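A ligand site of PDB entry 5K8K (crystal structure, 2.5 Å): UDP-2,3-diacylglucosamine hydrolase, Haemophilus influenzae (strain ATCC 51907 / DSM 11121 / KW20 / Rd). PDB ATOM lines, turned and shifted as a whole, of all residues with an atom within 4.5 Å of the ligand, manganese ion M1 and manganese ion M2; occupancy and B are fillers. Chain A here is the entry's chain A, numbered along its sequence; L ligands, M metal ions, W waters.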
ATOM      1  N   ASP A   9      26.649  18.079  15.645  1.00  0.00           N
ATOM      2  CA  ASP A   9      27.698  17.137  16.043  1.00  0.00           C
ATOM      3  C   ASP A   9      28.814  17.819  16.830  1.00  0.00           C
ATOM      4  O   ASP A   9      30.014  17.628  16.577  1.00  0.00           O
ATOM      5  CB  ASP A   9      28.259  16.391  14.829  1.00  0.00           C
ATOM      6  CG  ASP A   9      27.320  15.318  14.328  1.00  0.00           C
ATOM      7  OD1 ASP A   9      27.348  14.193  14.872  1.00  0.00           O
ATOM      8  OD2 ASP A   9      26.543  15.610  13.384  1.00  0.00           O
ATOM      9  N   HIS A  11      28.783  17.463  20.306  1.00  0.00           N
ATOM     10  CA  HIS A  11      28.940  16.552  21.439  1.00  0.00           C
ATOM     11  C   HIS A  11      29.630  17.261  22.618  1.00  0.00           C
ATOM     12  O   HIS A  11      30.696  16.868  23.085  1.00  0.00           O
ATOM     13  CB  HIS A  11      29.711  15.295  21.051  1.00  0.00           C
ATOM     14  CG  HIS A  11      29.415  14.790  19.667  1.00  0.00           C
ATOM     15  ND1 HIS A  11      30.143  15.184  18.566  1.00  0.00           N
ATOM     16  CD2 HIS A  11      28.480  13.926  19.209  1.00  0.00           C
ATOM     17  CE1 HIS A  11      29.671  14.581  17.487  1.00  0.00           C
ATOM     18  NE2 HIS A  11      28.655  13.815  17.848  1.00  0.00           N
ATOM     19  N   ASP A  42      22.895  16.199  17.967  1.00  0.00           N
ATOM     20  CA  ASP A  42      24.169  15.940  18.647  1.00  0.00           C
ATOM     21  C   ASP A  42      24.804  17.237  19.140  1.00  0.00           C
ATOM     22  O   ASP A  42      26.002  17.482  18.953  1.00  0.00           O
ATOM     23  CB  ASP A  42      25.127  15.142  17.757  1.00  0.00           C
ATOM     24  CG  ASP A  42      24.603  13.760  17.423  1.00  0.00           C
ATOM     25  OD1 ASP A  42      23.604  13.346  18.034  1.00  0.00           O
ATOM     26  OD2 ASP A  42      25.200  13.073  16.564  1.00  0.00           O
ATOM     27  N   PHE A  46      25.521  13.442  25.290  1.00  0.00           N
ATOM     28  CA  PHE A  46      24.336  12.609  25.473  1.00  0.00           C
ATOM     29  C   PHE A  46      23.316  13.417  26.251  1.00  0.00           C
ATOM     30  O   PHE A  46      23.652  14.380  26.949  1.00  0.00           O
ATOM     31  CB  PHE A  46      24.669  11.297  26.200  1.00  0.00           C
ATOM     32  CG  PHE A  46      25.222  11.475  27.577  1.00  0.00           C
ATOM     33  CD1 PHE A  46      24.381  11.596  28.671  1.00  0.00           C
ATOM     34  CD2 PHE A  46      26.601  11.505  27.786  1.00  0.00           C
ATOM     35  CE1 PHE A  46      24.897  11.765  29.943  1.00  0.00           C
ATOM     36  CE2 PHE A  46      27.117  11.674  29.058  1.00  0.00           C
ATOM     37  CZ  PHE A  46      26.260  11.806  30.136  1.00  0.00           C
ATOM     38  N   TRP A  47      22.054  13.016  26.130  1.00  0.00           N
ATOM     39  CA  TRP A  47      20.959  13.671  26.834  1.00  0.00           C
ATOM     40  C   TRP A  47      20.046  12.604  27.419  1.00  0.00           C
ATOM     41  O   TRP A  47      19.568  11.732  26.681  1.00  0.00           O
ATOM     42  CB  TRP A  47      20.163  14.589  25.908  1.00  0.00           C
ATOM     43  CG  TRP A  47      19.234  15.509  26.630  1.00  0.00           C
ATOM     44  CD1 TRP A  47      17.870  15.410  26.726  1.00  0.00           C
ATOM     45  CD2 TRP A  47      19.596  16.699  27.357  1.00  0.00           C
ATOM     46  NE1 TRP A  47      17.364  16.453  27.460  1.00  0.00           N
ATOM     47  CE2 TRP A  47      18.400  17.259  27.852  1.00  0.00           C
ATOM     48  CE3 TRP A  47      20.810  17.337  27.618  1.00  0.00           C
ATOM     49  CZ2 TRP A  47      18.382  18.429  28.619  1.00  0.00           C
ATOM     50  CZ3 TRP A  47      20.791  18.502  28.376  1.00  0.00           C
ATOM     51  CH2 TRP A  47      19.584  19.036  28.864  1.00  0.00           C
ATOM     52  N   ASN A  80      21.036  11.456  17.361  1.00  0.00           N
ATOM     53  CA  ASN A  80      21.061  10.164  18.047  1.00  0.00           C
ATOM     54  C   ASN A  80      21.575  10.271  19.483  1.00  0.00           C
ATOM     55  O   ASN A  80      21.204   9.445  20.317  1.00  0.00           O
ATOM     56  CB  ASN A  80      21.911   9.176  17.237  1.00  0.00           C
ATOM     57  CG  ASN A  80      23.288   9.723  16.895  1.00  0.00           C
ATOM     58  OD1 ASN A  80      23.425  10.588  16.030  1.00  0.00           O
ATOM     59  ND2 ASN A  80      24.309   9.205  17.556  1.00  0.00           N
ATOM     60  N   ARG A  81      22.393  11.278  19.785  1.00  0.00           N
ATOM     61  CA  ARG A  81      22.894  11.436  21.147  1.00  0.00           C
ATOM     62  C   ARG A  81      21.904  12.146  22.058  1.00  0.00           C
ATOM     63  O   ARG A  81      21.937  11.935  23.278  1.00  0.00           O
ATOM     64  CB  ARG A  81      24.212  12.214  21.148  1.00  0.00           C
ATOM     65  CG  ARG A  81      25.301  11.610  20.300  1.00  0.00           C
ATOM     66  CD  ARG A  81      25.946  10.409  20.971  1.00  0.00           C
ATOM     67  NE  ARG A  81      27.180  10.051  20.274  1.00  0.00           N
ATOM     68  CZ  ARG A  81      28.352  10.617  20.512  1.00  0.00           C
ATOM     69  NH1 ARG A  81      28.472  11.550  21.449  1.00  0.00           N
ATOM     70  NH2 ARG A  81      29.424  10.247  19.825  1.00  0.00           N
ATOM     71  N   PHE A  83      18.203  12.642  21.481  1.00  0.00           N
ATOM     72  CA  PHE A  83      16.836  12.577  20.988  1.00  0.00           C
ATOM     73  C   PHE A  83      15.793  12.739  22.080  1.00  0.00           C
ATOM     74  O   PHE A  83      14.602  12.851  21.761  1.00  0.00           O
ATOM     75  CB  PHE A  83      16.593  11.254  20.236  1.00  0.00           C
ATOM     76  CG  PHE A  83      16.853  10.024  21.069  1.00  0.00           C
ATOM     77  CD1 PHE A  83      18.129   9.505  21.177  1.00  0.00           C
ATOM     78  CD2 PHE A  83      15.813   9.390  21.730  1.00  0.00           C
ATOM     79  CE1 PHE A  83      18.371   8.388  21.948  1.00  0.00           C
ATOM     80  CE2 PHE A  83      16.050   8.261  22.498  1.00  0.00           C
ATOM     81  CZ  PHE A  83      17.322   7.758  22.608  1.00  0.00           C
ATOM     82  N   LEU A  84      16.186  12.763  23.351  1.00  0.00           N
ATOM     83  CA  LEU A  84      15.248  12.940  24.452  1.00  0.00           C
ATOM     84  C   LEU A  84      14.908  14.407  24.730  1.00  0.00           C
ATOM     85  O   LEU A  84      14.078  14.671  25.613  1.00  0.00           O
ATOM     86  CB  LEU A  84      15.806  12.300  25.725  1.00  0.00           C
ATOM     87  CG  LEU A  84      15.791  10.771  25.820  1.00  0.00           C
ATOM     88  CD1 LEU A  84      16.428  10.309  27.129  1.00  0.00           C
ATOM     89  CD2 LEU A  84      14.368  10.237  25.685  1.00  0.00           C
ATOM     90  N   HIS A 115      19.077  14.941  10.548  1.00  0.00           N
ATOM     91  CA  HIS A 115      20.313  14.708  11.278  1.00  0.00           C
ATOM     92  C   HIS A 115      21.302  13.915  10.438  1.00  0.00           C
ATOM     93  O   HIS A 115      22.502  14.227  10.434  1.00  0.00           O
ATOM     94  CB  HIS A 115      20.034  13.992  12.593  1.00  0.00           C
ATOM     95  CG  HIS A 115      21.271  13.730  13.398  1.00  0.00           C
ATOM     96  ND1 HIS A 115      22.160  14.730  13.727  1.00  0.00           N
ATOM     97  CD2 HIS A 115      21.786  12.594  13.902  1.00  0.00           C
ATOM     98  CE1 HIS A 115      23.162  14.223  14.408  1.00  0.00           C
ATOM     99  NE2 HIS A 115      22.961  12.919  14.534  1.00  0.00           N
ATOM    100  N   ASP A 123      23.142   0.240   8.114  1.00  0.00           N
ATOM    101  CA  ASP A 123      23.482  -0.059   9.508  1.00  0.00           C
ATOM    102  C   ASP A 123      22.247  -0.603  10.208  1.00  0.00           C
ATOM    103  O   ASP A 123      21.656   0.090  11.039  1.00  0.00           O
ATOM    104  CB  ASP A 123      23.996   1.191  10.210  1.00  0.00           C
ATOM    105  CG  ASP A 123      24.728   0.881  11.510  1.00  0.00           C
ATOM    106  OD1 ASP A 123      24.384  -0.114  12.169  1.00  0.00           O
ATOM    107  OD2 ASP A 123      25.633   1.663  11.879  1.00  0.00           O
ATOM    108  N   ALA A 125      21.827  -2.778  12.518  1.00  0.00           N
ATOM    109  CA  ALA A 125      21.899  -2.833  13.968  1.00  0.00           C
ATOM    110  C   ALA A 125      21.530  -1.497  14.581  1.00  0.00           C
ATOM    111  O   ALA A 125      20.765  -1.430  15.554  1.00  0.00           O
ATOM    112  CB  ALA A 125      23.290  -3.268  14.416  1.00  0.00           C
ATOM    113  N   TYR A 126      22.046  -0.398  14.021  1.00  0.00           N
ATOM    114  CA  TYR A 126      21.665   0.911  14.524  1.00  0.00           C
ATOM    115  C   TYR A 126      20.172   1.177  14.294  1.00  0.00           C
ATOM    116  O   TYR A 126      19.485   1.658  15.203  1.00  0.00           O
ATOM    117  CB  TYR A 126      22.485   2.023  13.870  1.00  0.00           C
ATOM    118  CG  TYR A 126      21.920   3.378  14.215  1.00  0.00           C
ATOM    119  CD1 TYR A 126      21.982   3.864  15.521  1.00  0.00           C
ATOM    120  CD2 TYR A 126      21.273   4.158  13.261  1.00  0.00           C
ATOM    121  CE1 TYR A 126      21.438   5.074  15.863  1.00  0.00           C
ATOM    122  CE2 TYR A 126      20.730   5.393  13.601  1.00  0.00           C
ATOM    123  CZ  TYR A 126      20.817   5.837  14.903  1.00  0.00           C
ATOM    124  OH  TYR A 126      20.289   7.061  15.258  1.00  0.00           O
ATOM    125  N   PHE A 129      18.016  -0.507  16.855  1.00  0.00           N
ATOM    126  CA  PHE A 129      18.125   0.211  18.114  1.00  0.00           C
ATOM    127  C   PHE A 129      17.390   1.545  18.069  1.00  0.00           C
ATOM    128  O   PHE A 129      16.810   1.967  19.075  1.00  0.00           O
ATOM    129  CB  PHE A 129      19.606   0.415  18.450  1.00  0.00           C
ATOM    130  CG  PHE A 129      19.853   1.375  19.571  1.00  0.00           C
ATOM    131  CD1 PHE A 129      19.623   1.004  20.891  1.00  0.00           C
ATOM    132  CD2 PHE A 129      20.312   2.658  19.323  1.00  0.00           C
ATOM    133  CE1 PHE A 129      19.860   1.898  21.924  1.00  0.00           C
ATOM    134  CE2 PHE A 129      20.538   3.552  20.346  1.00  0.00           C
ATOM    135  CZ  PHE A 129      20.314   3.166  21.649  1.00  0.00           C
ATOM    136  N   VAL A 133      14.323   2.886  20.940  1.00  0.00           N
ATOM    137  CA  VAL A 133      14.424   4.047  21.809  1.00  0.00           C
ATOM    138  C   VAL A 133      13.538   5.212  21.384  1.00  0.00           C
ATOM    139  O   VAL A 133      13.356   6.153  22.168  1.00  0.00           O
ATOM    140  CB  VAL A 133      15.896   4.534  21.892  1.00  0.00           C
ATOM    141  CG1 VAL A 133      16.771   3.445  22.461  1.00  0.00           C
ATOM    142  CG2 VAL A 133      16.391   4.940  20.520  1.00  0.00           C
ATOM    143  N   LEU A 138       8.398   3.594  26.124  1.00  0.00           N
ATOM    144  CA  LEU A 138       9.667   3.269  26.761  1.00  0.00           C
ATOM    145  C   LEU A 138      10.404   4.515  27.220  1.00  0.00           C
ATOM    146  O   LEU A 138      11.111   4.495  28.242  1.00  0.00           O
ATOM    147  CB  LEU A 138      10.530   2.443  25.810  1.00  0.00           C
ATOM    148  CG  LEU A 138      11.991   2.181  26.159  1.00  0.00           C
ATOM    149  CD1 LEU A 138      12.104   1.428  27.477  1.00  0.00           C
ATOM    150  CD2 LEU A 138      12.651   1.386  25.050  1.00  0.00           C
ATOM    151  N   GLN A 139      10.245   5.630  26.494  1.00  0.00           N
ATOM    152  CA  GLN A 139      10.866   6.885  26.932  1.00  0.00           C
ATOM    153  C   GLN A 139      10.244   7.378  28.231  1.00  0.00           C
ATOM    154  O   GLN A 139      10.950   7.889  29.102  1.00  0.00           O
ATOM    155  CB  GLN A 139      10.738   7.939  25.840  1.00  0.00           C
ATOM    156  CG  GLN A 139      11.536   7.600  24.599  1.00  0.00           C
ATOM    157  CD  GLN A 139      11.361   8.595  23.479  1.00  0.00           C
ATOM    158  OE1 GLN A 139      10.556   9.526  23.582  1.00  0.00           O
ATOM    159  NE2 GLN A 139      12.098   8.396  22.401  1.00  0.00           N
ATOM    160  N   PHE A 142      11.886   5.324  30.886  1.00  0.00           N
ATOM    161  CA  PHE A 142      13.270   5.706  31.136  1.00  0.00           C
ATOM    162  C   PHE A 142      13.354   6.968  31.985  1.00  0.00           C
ATOM    163  O   PHE A 142      14.148   7.045  32.926  1.00  0.00           O
ATOM    164  CB  PHE A 142      13.995   5.902  29.812  1.00  0.00           C
ATOM    165  CG  PHE A 142      15.442   6.302  29.960  1.00  0.00           C
ATOM    166  CD1 PHE A 142      16.398   5.352  30.250  1.00  0.00           C
ATOM    167  CD2 PHE A 142      15.831   7.617  29.785  1.00  0.00           C
ATOM    168  CE1 PHE A 142      17.732   5.719  30.378  1.00  0.00           C
ATOM    169  CE2 PHE A 142      17.153   7.981  29.917  1.00  0.00           C
ATOM    170  CZ  PHE A 142      18.109   7.032  30.207  1.00  0.00           C
ATOM    171  N   ALA A 154      23.345   5.835  30.232  1.00  0.00           N
ATOM    172  CA  ALA A 154      23.780   6.529  29.031  1.00  0.00           C
ATOM    173  C   ALA A 154      25.267   6.310  28.770  1.00  0.00           C
ATOM    174  O   ALA A 154      25.682   6.051  27.639  1.00  0.00           O
ATOM    175  CB  ALA A 154      23.471   8.023  29.137  1.00  0.00           C
ATOM    176  N   ILE A 157      25.557   2.772  27.518  1.00  0.00           N
ATOM    177  CA  ILE A 157      25.070   2.667  26.146  1.00  0.00           C
ATOM    178  C   ILE A 157      26.059   3.319  25.192  1.00  0.00           C
ATOM    179  O   ILE A 157      26.360   2.782  24.123  1.00  0.00           O
ATOM    180  CB  ILE A 157      23.658   3.269  26.014  1.00  0.00           C
ATOM    181  CG1 ILE A 157      22.619   2.317  26.612  1.00  0.00           C
ATOM    182  CG2 ILE A 157      23.331   3.558  24.554  1.00  0.00           C
ATOM    183  CD1 ILE A 157      21.194   2.790  26.451  1.00  0.00           C
ATOM    184  N   ARG A 158      26.579   4.490  25.578  1.00  0.00           N
ATOM    185  CA  ARG A 158      27.706   5.057  24.847  1.00  0.00           C
ATOM    186  C   ARG A 158      28.851   4.044  24.735  1.00  0.00           C
ATOM    187  O   ARG A 158      29.405   3.856  23.646  1.00  0.00           O
ATOM    188  CB  ARG A 158      28.204   6.338  25.523  1.00  0.00           C
ATOM    189  CG  ARG A 158      27.260   7.536  25.380  1.00  0.00           C
ATOM    190  CD  ARG A 158      27.105   8.007  23.940  1.00  0.00           C
ATOM    191  NE  ARG A 158      28.293   7.761  23.116  1.00  0.00           N
ATOM    192  CZ  ARG A 158      29.386   8.513  23.134  1.00  0.00           C
ATOM    193  NH1 ARG A 158      29.446   9.574  23.938  1.00  0.00           N
ATOM    194  NH2 ARG A 158      30.416   8.225  22.360  1.00  0.00           N
ATOM    195  N   LYS A 160      28.938   0.691  24.911  1.00  0.00           N
ATOM    196  CA  LYS A 160      28.658  -0.395  23.972  1.00  0.00           C
ATOM    197  C   LYS A 160      28.739   0.108  22.532  1.00  0.00           C
ATOM    198  O   LYS A 160      29.380  -0.530  21.685  1.00  0.00           O
ATOM    199  CB  LYS A 160      27.271  -1.002  24.234  1.00  0.00           C
ATOM    200  CG  LYS A 160      27.044  -2.277  23.428  1.00  0.00           C
ATOM    201  CD  LYS A 160      25.665  -2.881  23.640  1.00  0.00           C
ATOM    202  CE  LYS A 160      25.599  -4.334  23.154  1.00  0.00           C
ATOM    203  NZ  LYS A 160      26.030  -4.526  21.738  1.00  0.00           N
ATOM    204  N   SER A 161      28.102   1.244  22.246  1.00  0.00           N
ATOM    205  CA  SER A 161      28.117   1.790  20.897  1.00  0.00           C
ATOM    206  C   SER A 161      29.538   2.042  20.402  1.00  0.00           C
ATOM    207  O   SER A 161      29.814   1.900  19.216  1.00  0.00           O
ATOM    208  CB  SER A 161      27.296   3.081  20.855  1.00  0.00           C
ATOM    209  OG  SER A 161      27.272   3.648  19.547  1.00  0.00           O
ATOM    210  N   ASP A 164      30.621  -1.551  19.270  1.00  0.00           N
ATOM    211  CA  ASP A 164      29.969  -2.024  18.043  1.00  0.00           C
ATOM    212  C   ASP A 164      30.477  -1.303  16.803  1.00  0.00           C
ATOM    213  O   ASP A 164      30.530  -1.896  15.726  1.00  0.00           O
ATOM    214  CB  ASP A 164      28.451  -1.855  18.163  1.00  0.00           C
ATOM    215  CG  ASP A 164      27.864  -2.650  19.306  1.00  0.00           C
ATOM    216  OD1 ASP A 164      28.522  -2.768  20.358  1.00  0.00           O
ATOM    217  OD2 ASP A 164      26.733  -3.155  19.154  1.00  0.00           O
ATOM    218  N   LYS A 165      30.863  -0.024  16.929  1.00  0.00           N
ATOM    219  CA  LYS A 165      31.314   0.711  15.761  1.00  0.00           C
ATOM    220  C   LYS A 165      32.631   0.141  15.228  1.00  0.00           C
ATOM    221  O   LYS A 165      32.814   0.056  14.013  1.00  0.00           O
ATOM    222  CB  LYS A 165      31.458   2.204  16.095  1.00  0.00           C
ATOM    223  CG  LYS A 165      30.128   2.939  16.210  1.00  0.00           C
ATOM    224  CD  LYS A 165      30.268   4.421  15.866  1.00  0.00           C
ATOM    225  CE  LYS A 165      31.274   5.128  16.761  1.00  0.00           C
ATOM    226  NZ  LYS A 165      31.547   6.506  16.268  1.00  0.00           N
ATOM    227  N   LYS A 168      32.084  -2.583  12.859  1.00  0.00           N
ATOM    228  CA  LYS A 168      31.429  -2.237  11.619  1.00  0.00           C
ATOM    229  C   LYS A 168      32.423  -1.603  10.640  1.00  0.00           C
ATOM    230  O   LYS A 168      33.388  -0.946  11.047  1.00  0.00           O
ATOM    231  CB  LYS A 168      30.268  -1.257  11.846  1.00  0.00           C
ATOM    232  CG  LYS A 168      29.102  -1.821  12.651  1.00  0.00           C
ATOM    233  CD  LYS A 168      28.216  -0.704  13.208  1.00  0.00           C
ATOM    234  CE  LYS A 168      27.097  -1.277  14.058  1.00  0.00           C
ATOM    235  NZ  LYS A 168      26.446  -0.275  14.931  1.00  0.00           N
ATOM    236  N   MET A 173      28.203   2.539   7.849  1.00  0.00           N
ATOM    237  CA  MET A 173      27.997   3.592   8.841  1.00  0.00           C
ATOM    238  C   MET A 173      27.817   4.960   8.184  1.00  0.00           C
ATOM    239  O   MET A 173      27.654   5.970   8.868  1.00  0.00           O
ATOM    240  CB  MET A 173      29.147   3.638   9.846  1.00  0.00           C
ATOM    241  CG  MET A 173      29.089   2.530  10.883  1.00  0.00           C
ATOM    242  SD  MET A 173      30.237   2.829  12.429  1.00  0.00           S
ATOM    243  CE  MET A 173      31.952   2.906  11.508  1.00  0.00           C
ATOM    244  N   HIS A 196      25.869  14.024  11.504  1.00  0.00           N
ATOM    245  CA  HIS A 196      25.977  12.659  12.008  1.00  0.00           C
ATOM    246  C   HIS A 196      27.172  11.873  11.467  1.00  0.00           C
ATOM    247  O   HIS A 196      27.864  11.198  12.238  1.00  0.00           O
ATOM    248  CB  HIS A 196      24.693  11.871  11.740  1.00  0.00           C
ATOM    249  CG  HIS A 196      24.727  10.466  12.244  1.00  0.00           C
ATOM    250  ND1 HIS A 196      24.574  10.144  13.581  1.00  0.00           N
ATOM    251  CD2 HIS A 196      24.893   9.284  11.600  1.00  0.00           C
ATOM    252  CE1 HIS A 196      24.647   8.840  13.731  1.00  0.00           C
ATOM    253  NE2 HIS A 196      24.843   8.289  12.536  1.00  0.00           N
ATOM    254  N   HIS A 198      30.032  12.716  10.548  1.00  0.00           N
ATOM    255  CA  HIS A 198      31.313  13.196  11.062  1.00  0.00           C
ATOM    256  C   HIS A 198      32.212  13.818   9.989  1.00  0.00           C
ATOM    257  O   HIS A 198      33.075  14.641  10.307  1.00  0.00           O
ATOM    258  CB  HIS A 198      32.074  12.061  11.769  1.00  0.00           C
ATOM    259  CG  HIS A 198      31.253  11.301  12.757  1.00  0.00           C
ATOM    260  ND1 HIS A 198      30.646  11.896  13.844  1.00  0.00           N
ATOM    261  CD2 HIS A 198      30.958   9.979  12.839  1.00  0.00           C
ATOM    262  CE1 HIS A 198      29.997  10.969  14.538  1.00  0.00           C
ATOM    263  NE2 HIS A 198      30.168   9.809  13.950  1.00  0.00           N
HETATM  264  O1  LIG L   1      27.711   8.648  16.206  1.00  0.00           O
HETATM  265  P1  LIG L   1      27.783   7.648  17.334  1.00  0.00           P
HETATM  266  O2  LIG L   1      29.218   7.543  17.783  1.00  0.00           O
HETATM  267  O3  LIG L   1      26.903   8.079  18.489  1.00  0.00           O
HETATM  268  O4  LIG L   1      27.210   6.215  16.804  1.00  0.00           O
HETATM  269  C1  LIG L   1      25.961   6.241  16.228  1.00  0.00           C
HETATM  270  C2  LIG L   1      25.156   5.058  16.745  1.00  0.00           C
HETATM  271  N1  LIG L   1      25.176   5.066  18.226  1.00  0.00           N
HETATM  272  C3  LIG L   1      23.992   5.425  18.985  1.00  0.00           C
HETATM  273  C4  LIG L   1      24.018   5.408  20.513  1.00  0.00           C
HETATM  274  C5  LIG L   1      24.246   6.799  21.078  1.00  0.00           C
HETATM  275  O5  LIG L   1      25.582   7.171  20.877  1.00  0.00           O
HETATM  276  C6  LIG L   1      23.954   6.738  22.580  1.00  0.00           C
HETATM  277  C7  LIG L   1      23.398   8.068  23.054  1.00  0.00           C
HETATM  278  C8  LIG L   1      22.074   7.836  23.777  1.00  0.00           C
HETATM  279  C9  LIG L   1      22.338   7.873  25.282  1.00  0.00           C
HETATM  280  C10 LIG L   1      21.009   8.013  26.028  1.00  0.00           C
HETATM  281  C11 LIG L   1      20.029   6.968  25.518  1.00  0.00           C
HETATM  282  C12 LIG L   1      18.708   7.104  26.264  1.00  0.00           C
HETATM  283  C13 LIG L   1      17.946   5.788  26.175  1.00  0.00           C
HETATM  284  C14 LIG L   1      16.458   6.091  26.284  1.00  0.00           C
HETATM  285  C15 LIG L   1      15.650   4.839  25.957  1.00  0.00           C
HETATM  286  C16 LIG L   1      14.195   5.244  25.769  1.00  0.00           C
HETATM  287  O6  LIG L   1      22.990   5.721  18.423  1.00  0.00           O
HETATM  288  C17 LIG L   1      25.698   3.761  16.231  1.00  0.00           C
HETATM  289  C18 LIG L   1      25.825   3.783  14.756  1.00  0.00           C
HETATM  290  C19 LIG L   1      26.731   4.939  14.319  1.00  0.00           C
HETATM  291  O7  LIG L   1      26.119   6.214  14.763  1.00  0.00           O
HETATM  292  C20 LIG L   1      26.826   4.986  12.834  1.00  0.00           C
HETATM  293  O8  LIG L   1      25.572   5.245  12.290  1.00  0.00           O
HETATM  294  O9  LIG L   1      26.402   2.520  14.380  1.00  0.00           O
HETATM  295  O10 LIG L   1      24.803   2.658  16.578  1.00  0.00           O
HETATM  296  C21 LIG L   1      25.277   1.773  17.551  1.00  0.00           C
HETATM  297  O11 LIG L   1      26.447   1.541  17.629  1.00  0.00           O
HETATM  298  C22 LIG L   1      24.305   1.088  18.509  1.00  0.00           C
HETATM  299  C23 LIG L   1      24.749  -0.357  18.725  1.00  0.00           C
HETATM  300  O12 LIG L   1      24.980  -0.964  17.474  1.00  0.00           O
HETATM  301  C24 LIG L   1      23.686  -1.137  19.485  1.00  0.00           C
HETATM  302  C25 LIG L   1      23.256  -0.368  20.723  1.00  0.00           C
HETATM  303  C26 LIG L   1      22.740  -1.337  21.779  1.00  0.00           C
HETATM  304  C27 LIG L   1      22.923  -0.738  23.175  1.00  0.00           C
HETATM  305  C28 LIG L   1      21.860  -1.260  24.149  1.00  0.00           C
HETATM  306  C29 LIG L   1      20.580  -1.623  23.393  1.00  0.00           C
HETATM  307  C30 LIG L   1      19.438  -1.808  24.397  1.00  0.00           C
HETATM  308  C31 LIG L   1      18.205  -1.037  23.929  1.00  0.00           C
HETATM  309  C32 LIG L   1      17.800  -0.075  25.041  1.00  0.00           C
HETATM  310  C33 LIG L   1      16.277   0.031  25.140  1.00  0.00           C
HETATM  311  C34 LIG L   1      15.907   0.603  26.504  1.00  0.00           C
HETATM  312 MN    MN M   1      24.805  11.636  15.018  1.00  0.00          MN
HETATM  313 MN    MN M   2      27.461  12.564  16.294  1.00  0.00          MN
HETATM  314  O   HOH W   1      20.685   6.793  19.752  1.00  0.00           O
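NE2 of His 196 is in hydrogen-bond range of O8 of the ligand, at 3.1 Å.
An oxygen (O12) of the ligand lies within hydrogen-bond range of the side-chain carboxylate of Asp 164, 3.3 Å away.
O9 of the ligand sits at hydrogen-bond distance from OD2 of Asp 123, at 2.8 Å.
The side-chain hydroxyl of Ser 161 lies within hydrogen-bond range of a nitrogen (N1) of the ligand (2.9 Å).
NZ of Lys 165 is in salt-bridge range of O2 of the ligand.
An oxygen (O3) of the ligand lies within salt-bridge range of the guanidinium group (NE) of Arg 81, 2.7 Å away.
ND2 of Asn 80 lies within hydrogen-bond range of O3 of the ligand (3.0 Å).
The side-chain amino group of Lys 168 is in hydrogen-bond range of an oxygen (O9) of the ligand (2.8 Å).
OD1 of Asp 123 is in salt-bridge range of NZ of Lys 168 (3.5 Å).
The side-chain carboxylate (OD1) of Asp 42 lies within hydrogen-bond range of the backbone NH (N) of Arg 81 (3.0 Å).
The backbone carbonyl oxygen of Val 133 sits at hydrogen-bond distance from the side-chain amide nitrogen of Gln 139, 2.6 Å away.
O of Arg 81 lies within hydrogen-bond range of N of Trp 47 (3.1 Å).
The side-chain carboxylate (OD2) of Asp 164 is in salt-bridge range of the side-chain amino group (NZ) of Lys 160.
The side-chain carboxylate (OD1) of Asp 123 lies within hydrogen-bond range of the backbone NH (N) of Tyr 126.
The backbone NH of His 196 is in hydrogen-bond range of the side-chain carboxylate of Asp 9 (2.6 Å).
The backbone carbonyl oxygen (O) of His 196 lies close to a ring nitrogen (NE2) of His 198.
Residues that only touch the ligand: Tyr 126 (3.1 Å), Lys 160 (3.5 Å), Arg 158 (3.5 Å), His 198 (3.5 Å), Leu 138 (3.7 Å), Gln 139 (3.7 Å), Phe 129 (3.8 Å), Ile 157 (3.8 Å), Val 133 (3.8 Å), Phe 142 (3.8 Å), Met 173 (3.9 Å), Phe 83 (3.96 Å) and Ala 154 (3.97 Å).
Hydrophobic or aromatic side chains within 4 Å of the ligand: Phe 83, Tyr 126, Phe 129, Val 133, Leu 138, Phe 142, Ala 154, Ile 157, Met 173, His 196 and His 198.
Within 4 Å of the ligand: Asn 80, Arg 81, Phe 83, Asp 123, Tyr 126, Phe 129, Val 133, Leu 138, Gln 139, Phe 142, Ala 154, Ile 157, Arg 158, Lys 160, Ser 161, Asp 164, Lys 165, Lys 168, Met 173, His 196 and His 198.
The nearest printed residue that does not touch the ligand is Leu 84 (4.03 Å).
Of the 29 residues printed, 5 come within 4 Å of manganese ion M1.
CE1 of His 198 touches manganese ion M2, at 3.5 Å.
Within 4 Å of manganese ion M2: Asp 9, His 11, Asp 42 and His 198.
Along chain A the residues within 4 Å of manganese ion M2 span positions 9 to 198.
The nearest printed residue that does not touch manganese ion M2 is His 196 (4.3 Å).
Manganese ion M1 is bound by the side-chain amide oxygen (OD1) of Asn 80 (2.0 Å), a ring nitrogen (ND1) of His 196 (2.1 Å), the side-chain carboxylate (OD2) of Asp 42 (2.1 Å) and a ring nitrogen (NE2) of His 115 (2.3 Å).
OD1 of Asp 9 is bound to manganese ion M2 (2.2 Å).
NE2 of His 11 binds manganese ion M2 (2.3 Å).
OD2 of Asp 42 binds manganese ion M2 (2.3 Å).
Manganese ion M2 has three donor atoms within binding distance.
Water W1 bridges the backbone carbonyl oxygen (O) of Asn 80 (2.8 Å) and an oxygen (O6) of the ligand (2.9 Å).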
